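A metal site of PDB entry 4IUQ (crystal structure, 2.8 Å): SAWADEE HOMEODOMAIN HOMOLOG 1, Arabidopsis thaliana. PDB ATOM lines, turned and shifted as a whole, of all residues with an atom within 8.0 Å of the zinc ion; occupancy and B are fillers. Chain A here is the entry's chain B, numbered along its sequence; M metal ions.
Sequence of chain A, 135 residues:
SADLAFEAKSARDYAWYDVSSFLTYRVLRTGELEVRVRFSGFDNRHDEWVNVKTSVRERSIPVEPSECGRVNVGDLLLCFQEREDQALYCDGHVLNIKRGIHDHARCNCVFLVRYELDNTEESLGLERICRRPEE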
ATOM      1  N   VAL A  63      -5.347 -11.171  21.708  1.00  0.00           N
ATOM      2  CA  VAL A  63      -6.477 -11.517  20.860  1.00  0.00           C
ATOM      3  C   VAL A  63      -7.233 -12.726  21.453  1.00  0.00           C
ATOM      4  O   VAL A  63      -6.638 -13.783  21.732  1.00  0.00           O
ATOM      5  CB  VAL A  63      -6.026 -11.851  19.437  1.00  0.00           C
ATOM      6  CG1 VAL A  63      -7.216 -11.887  18.533  1.00  0.00           C
ATOM      7  CG2 VAL A  63      -5.107 -10.818  18.938  1.00  0.00           C
ATOM      8  N   GLU A  64      -8.536 -12.619  21.586  1.00  0.00           N
ATOM      9  CA  GLU A  64      -9.287 -13.738  22.061  1.00  0.00           C
ATOM     10  C   GLU A  64      -9.651 -14.698  20.946  1.00  0.00           C
ATOM     11  O   GLU A  64      -9.746 -14.314  19.825  1.00  0.00           O
ATOM     12  CB  GLU A  64     -10.486 -13.248  22.839  1.00  0.00           C
ATOM     13  CG  GLU A  64     -10.076 -12.329  23.937  1.00  0.00           C
ATOM     14  CD  GLU A  64      -9.285 -12.989  25.037  1.00  0.00           C
ATOM     15  OE1 GLU A  64      -9.643 -14.106  25.432  1.00  0.00           O
ATOM     16  OE2 GLU A  64      -8.303 -12.398  25.538  1.00  0.00           O
ATOM     17  N   PRO A  65      -9.816 -15.958  21.267  1.00  0.00           N
ATOM     18  CA  PRO A  65     -10.043 -16.903  20.182  1.00  0.00           C
ATOM     19  C   PRO A  65     -11.231 -16.495  19.293  1.00  0.00           C
ATOM     20  O   PRO A  65     -11.162 -16.625  18.063  1.00  0.00           O
ATOM     21  CB  PRO A  65     -10.347 -18.224  20.898  1.00  0.00           C
ATOM     22  CG  PRO A  65      -9.755 -18.079  22.233  1.00  0.00           C
ATOM     23  CD  PRO A  65      -9.786 -16.632  22.584  1.00  0.00           C
ATOM     24  N   SER A  66     -12.284 -15.984  19.906  1.00  0.00           N
ATOM     25  CA  SER A  66     -13.494 -15.669  19.162  1.00  0.00           C
ATOM     26  C   SER A  66     -13.289 -14.568  18.136  1.00  0.00           C
ATOM     27  O   SER A  66     -14.146 -14.363  17.294  1.00  0.00           O
ATOM     28  CB  SER A  66     -14.637 -15.298  20.108  1.00  0.00           C
ATOM     29  OG  SER A  66     -14.312 -14.160  20.895  1.00  0.00           O
ATOM     30  N   GLU A  67     -12.152 -13.865  18.194  1.00  0.00           N
ATOM     31  CA  GLU A  67     -11.894 -12.729  17.298  1.00  0.00           C
ATOM     32  C   GLU A  67     -10.566 -12.930  16.562  1.00  0.00           C
ATOM     33  O   GLU A  67      -9.997 -11.976  16.038  1.00  0.00           O
ATOM     34  CB  GLU A  67     -11.882 -11.399  18.078  1.00  0.00           C
ATOM     35  CG  GLU A  67     -10.557 -11.119  18.812  1.00  0.00           C
ATOM     36  CD  GLU A  67     -10.657 -10.182  20.033  1.00  0.00           C
ATOM     37  OE1 GLU A  67     -11.730  -9.563  20.221  1.00  0.00           O
ATOM     38  OE2 GLU A  67      -9.645 -10.071  20.799  1.00  0.00           O
ATOM     39  N   CYS A  68     -10.101 -14.165  16.483  1.00  0.00           N
ATOM     40  CA  CYS A  68      -8.865 -14.452  15.773  1.00  0.00           C
ATOM     41  C   CYS A  68      -8.928 -14.079  14.293  1.00  0.00           C
ATOM     42  O   CYS A  68      -7.895 -14.076  13.618  1.00  0.00           O
ATOM     43  CB  CYS A  68      -8.542 -15.935  15.851  1.00  0.00           C
ATOM     44  SG  CYS A  68      -9.444 -16.858  14.625  1.00  0.00           S
ATOM     45  N   GLY A  69     -10.131 -13.808  13.793  1.00  0.00           N
ATOM     46  CA  GLY A  69     -10.323 -13.465  12.381  1.00  0.00           C
ATOM     47  C   GLY A  69      -9.833 -12.070  11.998  1.00  0.00           C
ATOM     48  O   GLY A  69      -9.713 -11.753  10.812  1.00  0.00           O
ATOM     49  N   ILE A  97      -1.443 -17.504   7.071  1.00  0.00           N
ATOM     50  CA  ILE A  97      -2.329 -18.119   8.110  1.00  0.00           C
ATOM     51  C   ILE A  97      -3.016 -19.403   7.674  1.00  0.00           C
ATOM     52  O   ILE A  97      -3.755 -19.392   6.683  1.00  0.00           O
ATOM     53  CB  ILE A  97      -3.499 -17.183   8.512  1.00  0.00           C
ATOM     54  CG1 ILE A  97      -3.051 -15.723   8.608  1.00  0.00           C
ATOM     55  CG2 ILE A  97      -4.173 -17.699   9.779  1.00  0.00           C
ATOM     56  CD1 ILE A  97      -3.862 -14.924   9.544  1.00  0.00           C
ATOM     57  N   LYS A  98      -2.807 -20.482   8.428  1.00  0.00           N
ATOM     58  CA  LYS A  98      -3.594 -21.716   8.283  1.00  0.00           C
ATOM     59  C   LYS A  98      -4.656 -21.703   9.354  1.00  0.00           C
ATOM     60  O   LYS A  98      -4.368 -21.935  10.535  1.00  0.00           O
ATOM     61  CB  LYS A  98      -2.726 -22.964   8.483  1.00  0.00           C
ATOM     62  CG  LYS A  98      -1.570 -23.088   7.500  1.00  0.00           C
ATOM     63  CD  LYS A  98      -0.656 -24.309   7.828  1.00  0.00           C
ATOM     64  CE  LYS A  98       0.568 -24.341   6.902  1.00  0.00           C
ATOM     65  NZ  LYS A  98       0.261 -23.718   5.557  1.00  0.00           N
ATOM     66  N   ARG A  99      -5.893 -21.420   8.953  1.00  0.00           N
ATOM     67  CA  ARG A  99      -7.017 -21.325   9.855  1.00  0.00           C
ATOM     68  C   ARG A  99      -7.416 -22.738  10.240  1.00  0.00           C
ATOM     69  O   ARG A  99      -7.507 -23.593   9.376  1.00  0.00           O
ATOM     70  CB  ARG A  99      -8.193 -20.681   9.130  1.00  0.00           C
ATOM     71  CG  ARG A  99      -7.939 -19.267   8.668  1.00  0.00           C
ATOM     72  CD  ARG A  99      -8.114 -18.339   9.809  1.00  0.00           C
ATOM     73  NE  ARG A  99      -7.696 -16.960   9.561  1.00  0.00           N
ATOM     74  CZ  ARG A  99      -7.464 -16.113  10.551  1.00  0.00           C
ATOM     75  NH1 ARG A  99      -7.593 -16.523  11.817  1.00  0.00           N
ATOM     76  NH2 ARG A  99      -7.104 -14.861  10.304  1.00  0.00           N
ATOM     77  N   GLY A 100      -7.642 -22.977  11.540  1.00  0.00           N
ATOM     78  CA  GLY A 100      -8.073 -24.280  12.024  1.00  0.00           C
ATOM     79  C   GLY A 100      -9.561 -24.333  12.363  1.00  0.00           C
ATOM     80  O   GLY A 100     -10.235 -23.311  12.346  1.00  0.00           O
ATOM     81  N   ILE A 101     -10.049 -25.518  12.680  1.00  0.00           N
ATOM     82  CA  ILE A 101     -11.414 -25.686  13.128  1.00  0.00           C
ATOM     83  C   ILE A 101     -11.458 -25.648  14.619  1.00  0.00           C
ATOM     84  O   ILE A 101     -11.018 -26.537  15.281  1.00  0.00           O
ATOM     85  CB  ILE A 101     -12.065 -27.004  12.691  1.00  0.00           C
ATOM     86  CG1 ILE A 101     -11.713 -27.384  11.274  1.00  0.00           C
ATOM     87  CG2 ILE A 101     -13.550 -26.869  12.725  1.00  0.00           C
ATOM     88  CD1 ILE A 101     -12.282 -26.472  10.299  1.00  0.00           C
ATOM     89  N   HIS A 102     -12.021 -24.578  15.133  1.00  0.00           N
ATOM     90  CA  HIS A 102     -12.009 -24.357  16.563  1.00  0.00           C
ATOM     91  C   HIS A 102     -13.151 -23.414  16.930  1.00  0.00           C
ATOM     92  O   HIS A 102     -13.720 -22.748  16.051  1.00  0.00           O
ATOM     93  CB  HIS A 102     -10.653 -23.801  17.048  1.00  0.00           C
ATOM     94  CG  HIS A 102     -10.539 -22.315  16.955  1.00  0.00           C
ATOM     95  ND1 HIS A 102     -10.948 -21.469  17.958  1.00  0.00           N
ATOM     96  CD2 HIS A 102     -10.093 -21.520  15.946  1.00  0.00           C
ATOM     97  CE1 HIS A 102     -10.746 -20.221  17.590  1.00  0.00           C
ATOM     98  NE2 HIS A 102     -10.226 -20.215  16.375  1.00  0.00           N
ATOM     99  N   ASP A 103     -13.479 -23.408  18.209  1.00  0.00           N
ATOM    100  CA  ASP A 103     -14.586 -22.618  18.743  1.00  0.00           C
ATOM    101  C   ASP A 103     -14.048 -21.377  19.462  1.00  0.00           C
ATOM    102  O   ASP A 103     -12.978 -20.852  19.140  1.00  0.00           O
ATOM    103  CB  ASP A 103     -15.460 -23.487  19.664  1.00  0.00           C
ATOM    104  CG  ASP A 103     -14.729 -23.932  20.953  1.00  0.00           C
ATOM    105  OD1 ASP A 103     -13.471 -23.960  20.985  1.00  0.00           O
ATOM    106  OD2 ASP A 103     -15.426 -24.255  21.946  1.00  0.00           O
ATOM    107  N   ARG A 106     -10.489 -21.688  22.355  1.00  0.00           N
ATOM    108  CA  ARG A 106      -9.078 -21.750  22.049  1.00  0.00           C
ATOM    109  C   ARG A 106      -8.907 -21.841  20.558  1.00  0.00           C
ATOM    110  O   ARG A 106      -9.660 -22.530  19.877  1.00  0.00           O
ATOM    111  CB  ARG A 106      -8.449 -22.965  22.720  1.00  0.00           C
ATOM    112  CG  ARG A 106      -7.041 -23.272  22.320  1.00  0.00           C
ATOM    113  CD  ARG A 106      -6.229 -23.486  23.546  1.00  0.00           C
ATOM    114  NE  ARG A 106      -4.818 -23.482  23.190  1.00  0.00           N
ATOM    115  CZ  ARG A 106      -3.873 -22.971  23.970  1.00  0.00           C
ATOM    116  NH1 ARG A 106      -2.602 -22.995  23.589  1.00  0.00           N
ATOM    117  NH2 ARG A 106      -4.214 -22.403  25.111  1.00  0.00           N
ATOM    118  N   CYS A 107      -7.922 -21.135  20.040  1.00  0.00           N
ATOM    119  CA  CYS A 107      -7.750 -20.991  18.632  1.00  0.00           C
ATOM    120  C   CYS A 107      -6.604 -21.885  18.211  1.00  0.00           C
ATOM    121  O   CYS A 107      -5.518 -21.735  18.724  1.00  0.00           O
ATOM    122  CB  CYS A 107      -7.426 -19.528  18.355  1.00  0.00           C
ATOM    123  SG  CYS A 107      -6.761 -19.283  16.742  1.00  0.00           S
ATOM    124  N   ASN A 108      -6.825 -22.811  17.282  1.00  0.00           N
ATOM    125  CA  ASN A 108      -5.727 -23.619  16.737  1.00  0.00           C
ATOM    126  C   ASN A 108      -5.190 -23.172  15.363  1.00  0.00           C
ATOM    127  O   ASN A 108      -4.446 -23.928  14.729  1.00  0.00           O
ATOM    128  CB  ASN A 108      -6.110 -25.098  16.700  1.00  0.00           C
ATOM    129  CG  ASN A 108      -7.371 -25.361  15.926  1.00  0.00           C
ATOM    130  OD1 ASN A 108      -7.787 -24.566  15.066  1.00  0.00           O
ATOM    131  ND2 ASN A 108      -7.997 -26.478  16.217  1.00  0.00           N
ATOM    132  N   CYS A 109      -5.556 -21.956  14.941  1.00  0.00           N
ATOM    133  CA  CYS A 109      -4.933 -21.304  13.801  1.00  0.00           C
ATOM    134  C   CYS A 109      -3.409 -21.132  13.932  1.00  0.00           C
ATOM    135  O   CYS A 109      -2.854 -20.915  15.030  1.00  0.00           O
ATOM    136  CB  CYS A 109      -5.574 -19.956  13.554  1.00  0.00           C
ATOM    137  SG  CYS A 109      -7.326 -20.025  13.046  1.00  0.00           S
ATOM    138  N   VAL A 110      -2.720 -21.251  12.808  1.00  0.00           N
ATOM    139  CA  VAL A 110      -1.267 -21.141  12.758  1.00  0.00           C
ATOM    140  C   VAL A 110      -0.844 -19.901  11.948  1.00  0.00           C
ATOM    141  O   VAL A 110      -1.272 -19.680  10.796  1.00  0.00           O
ATOM    142  CB  VAL A 110      -0.597 -22.458  12.257  1.00  0.00           C
ATOM    143  CG1 VAL A 110       0.897 -22.326  12.248  1.00  0.00           C
ATOM    144  CG2 VAL A 110      -0.936 -23.605  13.182  1.00  0.00           C
ATOM    145  N   PHE A 111      -0.048 -19.066  12.611  1.00  0.00           N
ATOM    146  CA  PHE A 111       0.367 -17.784  12.101  1.00  0.00           C
ATOM    147  C   PHE A 111       1.864 -17.823  11.827  1.00  0.00           C
ATOM    148  O   PHE A 111       2.649 -17.911  12.777  1.00  0.00           O
ATOM    149  CB  PHE A 111       0.065 -16.707  13.119  1.00  0.00           C
ATOM    150  CG  PHE A 111      -1.424 -16.546  13.450  1.00  0.00           C
ATOM    151  CD1 PHE A 111      -2.242 -15.693  12.693  1.00  0.00           C
ATOM    152  CD2 PHE A 111      -2.006 -17.252  14.526  1.00  0.00           C
ATOM    153  CE1 PHE A 111      -3.602 -15.528  13.014  1.00  0.00           C
ATOM    154  CE2 PHE A 111      -3.368 -17.097  14.838  1.00  0.00           C
ATOM    155  CZ  PHE A 111      -4.155 -16.233  14.083  1.00  0.00           C
ATOM    156  N   LEU A 126      -2.214 -18.220  18.466  1.00  0.00           N
ATOM    157  CA  LEU A 126      -2.769 -16.960  18.974  1.00  0.00           C
ATOM    158  C   LEU A 126      -2.277 -16.680  20.393  1.00  0.00           C
ATOM    159  O   LEU A 126      -2.088 -15.523  20.781  1.00  0.00           O
ATOM    160  CB  LEU A 126      -4.296 -16.988  18.971  1.00  0.00           C
ATOM    161  CG  LEU A 126      -5.106 -15.689  19.072  1.00  0.00           C
ATOM    162  CD1 LEU A 126      -4.942 -14.816  17.848  1.00  0.00           C
ATOM    163  CD2 LEU A 126      -6.565 -15.982  19.275  1.00  0.00           C
HETATM  164 ZN    ZN M   1      -8.492 -18.944  15.137  1.00  0.00          ZN
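The guanidinium group of Arg 99 sits at hydrogen-bond distance from the backbone carbonyl oxygen of Cys 68.
ND1 of His 102 is in hydrogen-bond range of O of Arg 106, 2.5 Å away.
The guanidinium group (NH1) of Arg 99 lies close to the side-chain sulfur (SG) of Cys 109, 3.7 Å away.
The side-chain sulfur (SG) of Cys 109 lies close to the backbone NH (N) of Gly 100, at 3.3 Å.
Within 4 Å of the zinc ion: Cys 68, His 102, Cys 107 and Cys 109.
The nearest printed residue that does not touch the zinc ion is Arg 99 (4.2 Å).
The zinc ion is bound by the side-chain sulfur of Cys 68, the side-chain sulfur of Cys 107, a ring nitrogen (NE2) of His 102 and the side-chain sulfur of Cys 109.
The zinc ion has four donor atoms within binding distance.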
